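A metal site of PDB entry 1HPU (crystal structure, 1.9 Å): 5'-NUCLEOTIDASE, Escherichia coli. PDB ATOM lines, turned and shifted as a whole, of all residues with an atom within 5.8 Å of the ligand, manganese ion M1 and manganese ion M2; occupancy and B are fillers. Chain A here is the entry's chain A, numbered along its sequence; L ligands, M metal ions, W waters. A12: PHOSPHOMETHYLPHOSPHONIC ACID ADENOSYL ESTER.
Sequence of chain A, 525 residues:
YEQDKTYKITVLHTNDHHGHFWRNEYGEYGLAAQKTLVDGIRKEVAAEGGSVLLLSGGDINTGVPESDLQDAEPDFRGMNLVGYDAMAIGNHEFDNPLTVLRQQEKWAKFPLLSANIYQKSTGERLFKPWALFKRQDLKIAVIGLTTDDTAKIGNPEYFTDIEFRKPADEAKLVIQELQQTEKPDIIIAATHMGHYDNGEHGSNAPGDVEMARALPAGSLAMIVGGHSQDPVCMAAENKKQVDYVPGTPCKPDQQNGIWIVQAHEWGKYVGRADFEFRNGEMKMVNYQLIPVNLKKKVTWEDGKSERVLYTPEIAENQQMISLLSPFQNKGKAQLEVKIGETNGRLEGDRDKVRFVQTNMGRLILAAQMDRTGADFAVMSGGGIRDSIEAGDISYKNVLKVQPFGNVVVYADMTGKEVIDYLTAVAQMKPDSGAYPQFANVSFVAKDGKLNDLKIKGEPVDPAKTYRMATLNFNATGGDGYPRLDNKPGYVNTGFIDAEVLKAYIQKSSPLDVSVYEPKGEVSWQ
ND2 of Asn 406 lies within hydrogen-bond range of N1 of the ligand. A ring nitrogen (NE2) of His 92 lies within hydrogen-bond range of an oxygen (O3B) of the ligand (2.6 Å). The guanidinium group (NH1) of Arg 354 lies within salt-bridge range of an oxygen (O2A) of the ligand, at 3.3 Å. The side-chain carboxylate of Asp 95 is in hydrogen-bond range of a nitrogen (N6) of the ligand (3.2 Å). The guanidinium group (NH2) of Arg 385 lies within salt-bridge range of an oxygen (O3B) of the ligand. OD1 of Asp 479 is in hydrogen-bond range of O3' of the ligand (2.5 Å). NH1 of Arg 350 is in salt-bridge range of O1A of the ligand (2.6 Å). The backbone carbonyl oxygen (O) of Gly 433 is in hydrogen-bond range of an oxygen (O2') of the ligand, at 3.3 Å.
Water W1 bridges an oxygen (O2B) of the ligand and the backbone carbonyl oxygen of His 227. Water W3 bridges an oxygen (O3') of the ligand (2.9 Å) and the backbone NH of Gly 433 (3.2 Å). Water W7 bridges O of His 227 and O2B of the ligand. Water W6 bridges a nitrogen (N7) of the ligand (3.1 Å) and the side-chain carboxylate (OD1) of Asp 95 (3.3 Å). Water W2 lies within hydrogen-bond range of O of Asp 95 (2.9 Å), O of Phe 404 (3.0 Å) and N6 of the ligand (3.1 Å). Water W4 lies within hydrogen-bond range of NH1 of Arg 350 (3.0 Å) and O2B of the ligand (3.3 Å).
O1B of the ligand binds manganese ion M1, 2.2 Å away. OD1 of Asn 91 is bound to manganese ion M1 (2.2 Å). A ring nitrogen (NE2) of His 192 binds manganese ion M1. Water W1 binds manganese ion M1 (2.3 Å). ND1 of His 227 is bound to manganese ion M1, 2.3 Å away. OD2 of Asp 59 is bound to manganese ion M1 (2.4 Å). Manganese ion M1 has six donor atoms within binding distance.
Within 4 Å of manganese ion M2: Asp 16, His 18, Asp 59 and Gln 229.
OG of Ser 380 is in hydrogen-bond range of OD2 of Asp 479 (2.7 Å). The backbone NH (N) of His 92 is in hydrogen-bond range of the side-chain carboxylate (OD1) of Asp 59, 2.9 Å away. The backbone carbonyl oxygen of Gly 433 is in hydrogen-bond range of the backbone NH of Gly 382 (2.8 Å). O of Gly 433 is in hydrogen-bond range of N of Gly 381, 3.4 Å away. The backbone NH (N) of Thr 147 is in hydrogen-bond range of the backbone carbonyl oxygen (O) of His 192, at 2.8 Å. The backbone NH (N) of His 227 sits at hydrogen-bond distance from the side-chain carboxylate (OD2) of Asp 16 (2.7 Å). The guanidinium group (NE) of Arg 385 lies within hydrogen-bond range of the backbone carbonyl oxygen (O) of Gly 382, 2.8 Å away. ND1 of His 92 sits at hydrogen-bond distance from OD2 of Asp 95 (2.5 Å).
The backbone carbonyl oxygen (O) of Gly 382 sits close to an oxygen (O4') of the ligand, at 3.4 Å. O of Ile 153 touches C8 of the ligand, at 3.6 Å. Ser 380 touches the ligand. Gly 383 touches the ligand (N to O2', 3.9 Å). Phe 404 touches the ligand (CG to C6, 3.5 Å). Phe 473 touches the ligand. Within 4 Å of the ligand: Asp 59, Asn 91, His 92, Asp 95, Ile 153, His 227, Gln 229, Arg 350, Arg 354, Ser 380, Gly 382, Gly 383, Arg 385, Phe 404, Asn 406, Gly 433, Phe 473 and Asp 479. The nearest printed residue that does not touch the ligand is Ala 434 (4.2 Å).
Manganese ion M2 is bound by the side-chain carboxylate of Asp 16, water W1, a ring nitrogen (NE2) of His 18, the side-chain amide oxygen of Gln 229 and the side-chain carboxylate of Asp 59.
Within 4 Å of manganese ion M1: Asp 59, Asn 91, His 192 and His 227.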
ATOM      1  N   ASP A  16     -20.732  10.153   1.915  1.00  0.00           N
ATOM      2  CA  ASP A  16     -20.474   9.544   3.213  1.00  0.00           C
ATOM      3  C   ASP A  16     -21.106  10.290   4.393  1.00  0.00           C
ATOM      4  O   ASP A  16     -20.462  10.525   5.432  1.00  0.00           O
ATOM      5  CB  ASP A  16     -18.965   9.410   3.367  1.00  0.00           C
ATOM      6  CG  ASP A  16     -18.384   8.393   2.356  1.00  0.00           C
ATOM      7  OD1 ASP A  16     -18.406   7.194   2.690  1.00  0.00           O
ATOM      8  OD2 ASP A  16     -17.978   8.784   1.242  1.00  0.00           O
ATOM      9  N   HIS A  18     -23.479   9.241   6.361  1.00  0.00           N
ATOM     10  CA  HIS A  18     -23.494   8.390   7.547  1.00  0.00           C
ATOM     11  C   HIS A  18     -24.372   8.810   8.734  1.00  0.00           C
ATOM     12  O   HIS A  18     -23.891   8.866   9.864  1.00  0.00           O
ATOM     13  CB  HIS A  18     -22.062   8.168   8.039  1.00  0.00           C
ATOM     14  CG  HIS A  18     -21.295   7.184   7.188  1.00  0.00           C
ATOM     15  ND1 HIS A  18     -21.815   5.946   6.861  1.00  0.00           N
ATOM     16  CD2 HIS A  18     -20.088   7.270   6.576  1.00  0.00           C
ATOM     17  CE1 HIS A  18     -20.951   5.304   6.078  1.00  0.00           C
ATOM     18  NE2 HIS A  18     -19.904   6.083   5.897  1.00  0.00           N
ATOM     19  N   GLY A  58     -22.909   8.671  -1.907  1.00  0.00           N
ATOM     20  CA  GLY A  58     -23.406   7.536  -1.155  1.00  0.00           C
ATOM     21  C   GLY A  58     -22.975   7.301   0.278  1.00  0.00           C
ATOM     22  O   GLY A  58     -22.176   8.046   0.841  1.00  0.00           O
ATOM     23  N   ASP A  59     -23.451   6.202   0.851  1.00  0.00           N
ATOM     24  CA  ASP A  59     -23.178   5.848   2.245  1.00  0.00           C
ATOM     25  C   ASP A  59     -23.895   6.897   3.129  1.00  0.00           C
ATOM     26  O   ASP A  59     -23.272   7.587   3.929  1.00  0.00           O
ATOM     27  CB  ASP A  59     -21.676   5.844   2.603  1.00  0.00           C
ATOM     28  CG  ASP A  59     -21.055   4.423   2.593  1.00  0.00           C
ATOM     29  OD1 ASP A  59     -21.649   3.457   2.057  1.00  0.00           O
ATOM     30  OD2 ASP A  59     -19.942   4.281   3.120  1.00  0.00           O
ATOM     31  N   GLY A  90     -23.886   3.367  -1.928  1.00  0.00           N
ATOM     32  CA  GLY A  90     -22.651   3.070  -1.221  1.00  0.00           C
ATOM     33  C   GLY A  90     -22.795   1.687  -0.613  1.00  0.00           C
ATOM     34  O   GLY A  90     -23.883   1.116  -0.664  1.00  0.00           O
ATOM     35  N   ASN A  91     -21.728   1.136  -0.036  1.00  0.00           N
ATOM     36  CA  ASN A  91     -21.825  -0.193   0.535  1.00  0.00           C
ATOM     37  C   ASN A  91     -22.725  -0.226   1.737  1.00  0.00           C
ATOM     38  O   ASN A  91     -23.423  -1.233   1.971  1.00  0.00           O
ATOM     39  CB  ASN A  91     -20.448  -0.764   0.884  1.00  0.00           C
ATOM     40  CG  ASN A  91     -19.598   0.189   1.720  1.00  0.00           C
ATOM     41  OD1 ASN A  91     -19.263   1.270   1.268  1.00  0.00           O
ATOM     42  ND2 ASN A  91     -19.231  -0.235   2.916  1.00  0.00           N
ATOM     43  N   HIS A  92     -22.736   0.860   2.510  1.00  0.00           N
ATOM     44  CA  HIS A  92     -23.564   0.894   3.684  1.00  0.00           C
ATOM     45  C   HIS A  92     -25.056   0.930   3.446  1.00  0.00           C
ATOM     46  O   HIS A  92     -25.828   0.779   4.395  1.00  0.00           O
ATOM     47  CB  HIS A  92     -23.108   2.004   4.640  1.00  0.00           C
ATOM     48  CG  HIS A  92     -21.881   1.650   5.401  1.00  0.00           C
ATOM     49  ND1 HIS A  92     -21.906   0.855   6.520  1.00  0.00           N
ATOM     50  CD2 HIS A  92     -20.570   1.870   5.127  1.00  0.00           C
ATOM     51  CE1 HIS A  92     -20.670   0.587   6.904  1.00  0.00           C
ATOM     52  NE2 HIS A  92     -19.837   1.199   6.074  1.00  0.00           N
ATOM     53  N   PHE A  94     -26.405  -1.302   2.170  1.00  0.00           N
ATOM     54  CA  PHE A  94     -26.694  -2.736   2.257  1.00  0.00           C
ATOM     55  C   PHE A  94     -26.482  -3.206   3.683  1.00  0.00           C
ATOM     56  O   PHE A  94     -26.305  -4.404   3.933  1.00  0.00           O
ATOM     57  CB  PHE A  94     -25.769  -3.519   1.318  1.00  0.00           C
ATOM     58  CG  PHE A  94     -26.046  -3.255  -0.121  1.00  0.00           C
ATOM     59  CD1 PHE A  94     -27.123  -3.872  -0.768  1.00  0.00           C
ATOM     60  CD2 PHE A  94     -25.278  -2.348  -0.837  1.00  0.00           C
ATOM     61  CE1 PHE A  94     -27.431  -3.573  -2.103  1.00  0.00           C
ATOM     62  CE2 PHE A  94     -25.570  -2.041  -2.171  1.00  0.00           C
ATOM     63  CZ  PHE A  94     -26.641  -2.646  -2.798  1.00  0.00           C
ATOM     64  N   ASP A  95     -26.497  -2.266   4.623  1.00  0.00           N
ATOM     65  CA  ASP A  95     -26.337  -2.628   6.034  1.00  0.00           C
ATOM     66  C   ASP A  95     -27.673  -3.207   6.531  1.00  0.00           C
ATOM     67  O   ASP A  95     -27.748  -3.863   7.569  1.00  0.00           O
ATOM     68  CB  ASP A  95     -25.975  -1.409   6.894  1.00  0.00           C
ATOM     69  CG  ASP A  95     -24.497  -1.030   6.808  1.00  0.00           C
ATOM     70  OD1 ASP A  95     -23.710  -1.760   6.171  1.00  0.00           O
ATOM     71  OD2 ASP A  95     -24.128   0.017   7.410  1.00  0.00           O
ATOM     72  N   THR A 147     -18.543   0.382  -5.106  1.00  0.00           N
ATOM     73  CA  THR A 147     -17.350  -0.444  -4.950  1.00  0.00           C
ATOM     74  C   THR A 147     -17.689  -1.928  -4.904  1.00  0.00           C
ATOM     75  O   THR A 147     -18.635  -2.340  -4.233  1.00  0.00           O
ATOM     76  CB  THR A 147     -16.585  -0.148  -3.661  1.00  0.00           C
ATOM     77  OG1 THR A 147     -15.512  -1.090  -3.542  1.00  0.00           O
ATOM     78  CG2 THR A 147     -17.468  -0.282  -2.442  1.00  0.00           C
ATOM     79  N   ILE A 153     -16.818  -6.851   2.335  1.00  0.00           N
ATOM     80  CA  ILE A 153     -16.750  -6.212   3.661  1.00  0.00           C
ATOM     81  C   ILE A 153     -18.112  -6.002   4.308  1.00  0.00           C
ATOM     82  O   ILE A 153     -18.222  -5.397   5.376  1.00  0.00           O
ATOM     83  CB  ILE A 153     -16.100  -4.813   3.571  1.00  0.00           C
ATOM     84  CG1 ILE A 153     -16.978  -3.888   2.716  1.00  0.00           C
ATOM     85  CG2 ILE A 153     -14.690  -4.925   3.030  1.00  0.00           C
ATOM     86  CD1 ILE A 153     -16.531  -2.438   2.649  1.00  0.00           C
ATOM     87  N   GLY A 154     -19.158  -6.470   3.642  1.00  0.00           N
ATOM     88  CA  GLY A 154     -20.510  -6.331   4.170  1.00  0.00           C
ATOM     89  C   GLY A 154     -21.007  -7.655   4.705  1.00  0.00           C
ATOM     90  O   GLY A 154     -20.276  -8.644   4.686  1.00  0.00           O
ATOM     91  N   ASN A 155     -22.251  -7.685   5.167  1.00  0.00           N
ATOM     92  CA  ASN A 155     -22.821  -8.903   5.721  1.00  0.00           C
ATOM     93  C   ASN A 155     -23.218  -9.862   4.614  1.00  0.00           C
ATOM     94  O   ASN A 155     -24.136  -9.600   3.871  1.00  0.00           O
ATOM     95  CB  ASN A 155     -24.054  -8.567   6.569  1.00  0.00           C
ATOM     96  CG  ASN A 155     -24.585  -9.774   7.322  1.00  0.00           C
ATOM     97  OD1 ASN A 155     -23.948 -10.288   8.238  1.00  0.00           O
ATOM     98  ND2 ASN A 155     -25.760 -10.241   6.922  1.00  0.00           N
ATOM     99  N   HIS A 192     -19.071   5.262  -5.418  1.00  0.00           N
ATOM    100  CA  HIS A 192     -18.717   4.971  -4.047  1.00  0.00           C
ATOM    101  C   HIS A 192     -17.593   3.960  -4.182  1.00  0.00           C
ATOM    102  O   HIS A 192     -17.779   2.764  -3.929  1.00  0.00           O
ATOM    103  CB  HIS A 192     -19.886   4.357  -3.285  1.00  0.00           C
ATOM    104  CG  HIS A 192     -19.662   4.376  -1.804  1.00  0.00           C
ATOM    105  ND1 HIS A 192     -19.762   5.528  -1.062  1.00  0.00           N
ATOM    106  CD2 HIS A 192     -19.185   3.417  -0.973  1.00  0.00           C
ATOM    107  CE1 HIS A 192     -19.362   5.294   0.168  1.00  0.00           C
ATOM    108  NE2 HIS A 192     -19.003   4.023   0.259  1.00  0.00           N
ATOM    109  N   ASN A 204      -7.452  -2.801  -1.094  1.00  0.00           N
ATOM    110  CA  ASN A 204      -8.806  -2.336  -1.372  1.00  0.00           C
ATOM    111  C   ASN A 204      -9.114  -2.499  -2.846  1.00  0.00           C
ATOM    112  O   ASN A 204      -8.219  -2.456  -3.688  1.00  0.00           O
ATOM    113  CB  ASN A 204      -8.967  -0.849  -1.027  1.00  0.00           C
ATOM    114  CG  ASN A 204      -8.687  -0.550   0.433  1.00  0.00           C
ATOM    115  OD1 ASN A 204      -9.434  -0.976   1.310  1.00  0.00           O
ATOM    116  ND2 ASN A 204      -7.616   0.184   0.691  1.00  0.00           N
ATOM    117  N   HIS A 227     -16.605   6.950  -0.226  1.00  0.00           N
ATOM    118  CA  HIS A 227     -16.072   5.727   0.380  1.00  0.00           C
ATOM    119  C   HIS A 227     -14.743   5.841   1.151  1.00  0.00           C
ATOM    120  O   HIS A 227     -14.663   5.416   2.302  1.00  0.00           O
ATOM    121  CB  HIS A 227     -15.948   4.653  -0.729  1.00  0.00           C
ATOM    122  CG  HIS A 227     -15.600   3.296  -0.214  1.00  0.00           C
ATOM    123  ND1 HIS A 227     -16.311   2.664   0.777  1.00  0.00           N
ATOM    124  CD2 HIS A 227     -14.606   2.434  -0.562  1.00  0.00           C
ATOM    125  CE1 HIS A 227     -15.789   1.486   1.030  1.00  0.00           C
ATOM    126  NE2 HIS A 227     -14.751   1.316   0.222  1.00  0.00           N
ATOM    127  N   GLN A 229     -13.531   8.448   2.192  1.00  0.00           N
ATOM    128  CA  GLN A 229     -13.790   9.574   3.078  1.00  0.00           C
ATOM    129  C   GLN A 229     -12.617  10.512   3.196  1.00  0.00           C
ATOM    130  O   GLN A 229     -11.981  10.633   4.243  1.00  0.00           O
ATOM    131  CB  GLN A 229     -14.262   9.072   4.453  1.00  0.00           C
ATOM    132  CG  GLN A 229     -15.678   8.510   4.307  1.00  0.00           C
ATOM    133  CD  GLN A 229     -16.202   7.805   5.563  1.00  0.00           C
ATOM    134  OE1 GLN A 229     -16.734   6.687   5.486  1.00  0.00           O
ATOM    135  NE2 GLN A 229     -16.045   8.434   6.708  1.00  0.00           N
ATOM    136  N   ARG A 350     -10.587   4.048  15.557  1.00  0.00           N
ATOM    137  CA  ARG A 350     -10.143   3.304  14.380  1.00  0.00           C
ATOM    138  C   ARG A 350      -8.640   3.042  14.333  1.00  0.00           C
ATOM    139  O   ARG A 350      -8.217   1.922  14.006  1.00  0.00           O
ATOM    140  CB  ARG A 350     -10.579   4.047  13.110  1.00  0.00           C
ATOM    141  CG  ARG A 350     -10.092   3.430  11.814  1.00  0.00           C
ATOM    142  CD  ARG A 350     -10.876   4.013  10.647  1.00  0.00           C
ATOM    143  NE  ARG A 350     -10.366   3.582   9.352  1.00  0.00           N
ATOM    144  CZ  ARG A 350     -11.140   3.173   8.353  1.00  0.00           C
ATOM    145  NH1 ARG A 350     -12.460   3.142   8.516  1.00  0.00           N
ATOM    146  NH2 ARG A 350     -10.607   2.820   7.191  1.00  0.00           N
ATOM    147  N   ARG A 354      -8.123  -1.382  14.774  1.00  0.00           N
ATOM    148  CA  ARG A 354      -7.773  -2.072  13.546  1.00  0.00           C
ATOM    149  C   ARG A 354      -6.260  -2.289  13.496  1.00  0.00           C
ATOM    150  O   ARG A 354      -5.726  -2.700  12.456  1.00  0.00           O
ATOM    151  CB  ARG A 354      -8.199  -1.251  12.322  1.00  0.00           C
ATOM    152  CG  ARG A 354      -9.688  -0.956  12.223  1.00  0.00           C
ATOM    153  CD  ARG A 354     -10.051  -0.497  10.811  1.00  0.00           C
ATOM    154  NE  ARG A 354     -11.465  -0.133  10.725  1.00  0.00           N
ATOM    155  CZ  ARG A 354     -12.140   0.031   9.590  1.00  0.00           C
ATOM    156  NH1 ARG A 354     -11.526  -0.132   8.421  1.00  0.00           N
ATOM    157  NH2 ARG A 354     -13.426   0.368   9.628  1.00  0.00           N
ATOM    158  N   SER A 380     -14.178  -8.584  14.131  1.00  0.00           N
ATOM    159  CA  SER A 380     -13.378  -7.664  13.327  1.00  0.00           C
ATOM    160  C   SER A 380     -13.237  -6.300  14.020  1.00  0.00           C
ATOM    161  O   SER A 380     -14.219  -5.788  14.558  1.00  0.00           O
ATOM    162  CB  SER A 380     -14.057  -7.422  11.983  1.00  0.00           C
ATOM    163  OG  SER A 380     -14.067  -8.606  11.188  1.00  0.00           O
ATOM    164  N   GLY A 381     -12.044  -5.720  13.984  1.00  0.00           N
ATOM    165  CA  GLY A 381     -11.838  -4.407  14.567  1.00  0.00           C
ATOM    166  C   GLY A 381     -12.733  -3.390  13.858  1.00  0.00           C
ATOM    167  O   GLY A 381     -13.158  -2.380  14.443  1.00  0.00           O
ATOM    168  N   GLY A 382     -13.023  -3.671  12.602  1.00  0.00           N
ATOM    169  CA  GLY A 382     -13.881  -2.796  11.823  1.00  0.00           C
ATOM    170  C   GLY A 382     -15.305  -2.747  12.358  1.00  0.00           C
ATOM    171  O   GLY A 382     -16.071  -1.858  12.011  1.00  0.00           O
ATOM    172  N   GLY A 383     -15.648  -3.723  13.211  1.00  0.00           N
ATOM    173  CA  GLY A 383     -16.982  -3.770  13.794  1.00  0.00           C
ATOM    174  C   GLY A 383     -17.149  -2.833  14.993  1.00  0.00           C
ATOM    175  O   GLY A 383     -18.254  -2.652  15.473  1.00  0.00           O
ATOM    176  N   ARG A 385     -16.953   0.860  16.107  1.00  0.00           N
ATOM    177  CA  ARG A 385     -16.987   2.172  15.487  1.00  0.00           C
ATOM    178  C   ARG A 385     -16.934   3.412  16.382  1.00  0.00           C
ATOM    179  O   ARG A 385     -17.124   4.524  15.915  1.00  0.00           O
ATOM    180  CB  ARG A 385     -18.219   2.233  14.563  1.00  0.00           C
ATOM    181  CG  ARG A 385     -18.147   1.296  13.332  1.00  0.00           C
ATOM    182  CD  ARG A 385     -16.850   1.538  12.542  1.00  0.00           C
ATOM    183  NE  ARG A 385     -16.752   0.802  11.280  1.00  0.00           N
ATOM    184  CZ  ARG A 385     -17.089   1.281  10.098  1.00  0.00           C
ATOM    185  NH1 ARG A 385     -17.566   2.518   9.988  1.00  0.00           N
ATOM    186  NH2 ARG A 385     -16.915   0.549   9.010  1.00  0.00           N
ATOM    187  N   PHE A 404     -24.184  -1.713  13.438  1.00  0.00           N
ATOM    188  CA  PHE A 404     -24.637  -2.543  12.319  1.00  0.00           C
ATOM    189  C   PHE A 404     -25.789  -3.483  12.550  1.00  0.00           C
ATOM    190  O   PHE A 404     -26.328  -4.058  11.592  1.00  0.00           O
ATOM    191  CB  PHE A 404     -23.444  -3.307  11.750  1.00  0.00           C
ATOM    192  CG  PHE A 404     -22.306  -2.426  11.387  1.00  0.00           C
ATOM    193  CD1 PHE A 404     -22.482  -1.409  10.450  1.00  0.00           C
ATOM    194  CD2 PHE A 404     -21.069  -2.584  11.988  1.00  0.00           C
ATOM    195  CE1 PHE A 404     -21.427  -0.560  10.118  1.00  0.00           C
ATOM    196  CE2 PHE A 404     -20.006  -1.754  11.669  1.00  0.00           C
ATOM    197  CZ  PHE A 404     -20.173  -0.740  10.737  1.00  0.00           C
ATOM    198  N   ASN A 406     -25.587  -6.310  13.952  1.00  0.00           N
ATOM    199  CA  ASN A 406     -25.133  -7.693  13.766  1.00  0.00           C
ATOM    200  C   ASN A 406     -25.762  -8.525  14.905  1.00  0.00           C
ATOM    201  O   ASN A 406     -26.192  -7.984  15.936  1.00  0.00           O
ATOM    202  CB  ASN A 406     -23.612  -7.815  13.843  1.00  0.00           C
ATOM    203  CG  ASN A 406     -22.900  -7.269  12.607  1.00  0.00           C
ATOM    204  OD1 ASN A 406     -21.662  -7.220  12.558  1.00  0.00           O
ATOM    205  ND2 ASN A 406     -23.668  -6.870  11.609  1.00  0.00           N
ATOM    206  N   SER A 432      -6.678  -2.625   8.777  1.00  0.00           N
ATOM    207  CA  SER A 432      -7.743  -3.218   7.979  1.00  0.00           C
ATOM    208  C   SER A 432      -8.954  -3.478   8.865  1.00  0.00           C
ATOM    209  O   SER A 432      -8.788  -3.806  10.035  1.00  0.00           O
ATOM    210  CB  SER A 432      -7.313  -4.549   7.383  1.00  0.00           C
ATOM    211  OG  SER A 432      -8.451  -5.215   6.866  1.00  0.00           O
ATOM    212  N   GLY A 433     -10.143  -3.359   8.300  1.00  0.00           N
ATOM    213  CA  GLY A 433     -11.341  -3.616   9.081  1.00  0.00           C
ATOM    214  C   GLY A 433     -11.345  -5.044   9.584  1.00  0.00           C
ATOM    215  O   GLY A 433     -11.951  -5.347  10.618  1.00  0.00           O
ATOM    216  N   ALA A 434     -10.631  -5.916   8.872  1.00  0.00           N
ATOM    217  CA  ALA A 434     -10.559  -7.335   9.229  1.00  0.00           C
ATOM    218  C   ALA A 434      -9.615  -7.705  10.379  1.00  0.00           C
ATOM    219  O   ALA A 434      -9.677  -8.832  10.862  1.00  0.00           O
ATOM    220  CB  ALA A 434     -10.198  -8.162   7.978  1.00  0.00           C
ATOM    221  N   PHE A 473     -21.916 -11.654  11.157  1.00  0.00           N
ATOM    222  CA  PHE A 473     -21.106 -11.036  10.133  1.00  0.00           C
ATOM    223  C   PHE A 473     -19.804 -11.830   9.892  1.00  0.00           C
ATOM    224  O   PHE A 473     -19.502 -12.177   8.767  1.00  0.00           O
ATOM    225  CB  PHE A 473     -20.739  -9.588  10.506  1.00  0.00           C
ATOM    226  CG  PHE A 473     -19.712  -8.979   9.574  1.00  0.00           C
ATOM    227  CD1 PHE A 473     -20.092  -8.419   8.361  1.00  0.00           C
ATOM    228  CD2 PHE A 473     -18.357  -9.009   9.906  1.00  0.00           C
ATOM    229  CE1 PHE A 473     -19.121  -7.899   7.475  1.00  0.00           C
ATOM    230  CE2 PHE A 473     -17.397  -8.493   9.035  1.00  0.00           C
ATOM    231  CZ  PHE A 473     -17.770  -7.938   7.826  1.00  0.00           C
ATOM    232  N   ASP A 479     -15.498 -10.174   6.052  1.00  0.00           N
ATOM    233  CA  ASP A 479     -14.086  -9.757   6.174  1.00  0.00           C
ATOM    234  C   ASP A 479     -13.115 -10.899   5.832  1.00  0.00           C
ATOM    235  O   ASP A 479     -11.936 -10.865   6.196  1.00  0.00           O
ATOM    236  CB  ASP A 479     -13.776  -9.225   7.579  1.00  0.00           C
ATOM    237  CG  ASP A 479     -13.996  -7.728   7.690  1.00  0.00           C
ATOM    238  OD1 ASP A 479     -14.031  -7.056   6.640  1.00  0.00           O
ATOM    239  OD2 ASP A 479     -14.136  -7.214   8.822  1.00  0.00           O
HETATM  240  PB  A12 L   1     -16.551   1.716   4.898  1.00  0.00           P
HETATM  241  O1B A12 L   1     -17.467   1.760   3.713  1.00  0.00           O
HETATM  242  O2B A12 L   1     -16.177   3.099   5.333  1.00  0.00           O
HETATM  243  O3B A12 L   1     -17.200   1.040   6.048  1.00  0.00           O
HETATM  244  PA  A12 L   1     -13.945   0.622   5.864  1.00  0.00           P
HETATM  245  O1A A12 L   1     -13.679   1.935   6.516  1.00  0.00           O
HETATM  246  O2A A12 L   1     -12.692   0.001   5.373  1.00  0.00           O
HETATM  247  C3A A12 L   1     -15.057   0.854   4.506  1.00  0.00           C
HETATM  248  O5' A12 L   1     -14.633  -0.328   6.946  1.00  0.00           O
HETATM  249  C5' A12 L   1     -15.030  -1.619   6.538  1.00  0.00           C
HETATM  250  C4' A12 L   1     -15.056  -2.562   7.711  1.00  0.00           C
HETATM  251  O4' A12 L   1     -16.144  -2.200   8.609  1.00  0.00           O
HETATM  252  C3' A12 L   1     -15.333  -3.991   7.307  1.00  0.00           C
HETATM  253  O3' A12 L   1     -14.101  -4.602   6.946  1.00  0.00           O
HETATM  254  C2' A12 L   1     -15.954  -4.570   8.574  1.00  0.00           C
HETATM  255  O2' A12 L   1     -14.981  -4.869   9.537  1.00  0.00           O
HETATM  256  C1' A12 L   1     -16.787  -3.378   9.085  1.00  0.00           C
HETATM  257  N9  A12 L   1     -18.172  -3.383   8.604  1.00  0.00           N
HETATM  258  C8  A12 L   1     -18.702  -2.606   7.610  1.00  0.00           C
HETATM  259  N7  A12 L   1     -19.981  -2.820   7.382  1.00  0.00           N
HETATM  260  C5  A12 L   1     -20.307  -3.801   8.309  1.00  0.00           C
HETATM  261  C6  A12 L   1     -21.522  -4.438   8.593  1.00  0.00           C
HETATM  262  N6  A12 L   1     -22.661  -4.178   7.970  1.00  0.00           N
HETATM  263  N1  A12 L   1     -21.521  -5.383   9.568  1.00  0.00           N
HETATM  264  C2  A12 L   1     -20.376  -5.632  10.212  1.00  0.00           C
HETATM  265  N3  A12 L   1     -19.170  -5.073  10.049  1.00  0.00           N
HETATM  266  C4  A12 L   1     -19.205  -4.162   9.065  1.00  0.00           C
HETATM  267 MN    MN M   1     -18.206   3.020   2.094  1.00  0.00          MN
HETATM  268 MN    MN M   2     -18.435   5.779   4.194  1.00  0.00          MN
HETATM  269  O   HOH W   1     -16.904   4.433   3.387  1.00  0.00           O
HETATM  270  O   HOH W   2     -25.524  -5.079   8.881  1.00  0.00           O
HETATM  271  O   HOH W   3     -11.913  -3.202   5.690  1.00  0.00           O
HETATM  272  O   HOH W   4     -14.960   4.760   7.941  1.00  0.00           O
HETATM  273  O   HOH W   5     -17.207  -6.170  11.478  1.00  0.00           O
HETATM  274  O   HOH W   6     -21.112  -2.822   4.509  1.00  0.00           O
HETATM  275  O   HOH W   7     -13.589   4.623   4.693  1.00  0.00           O
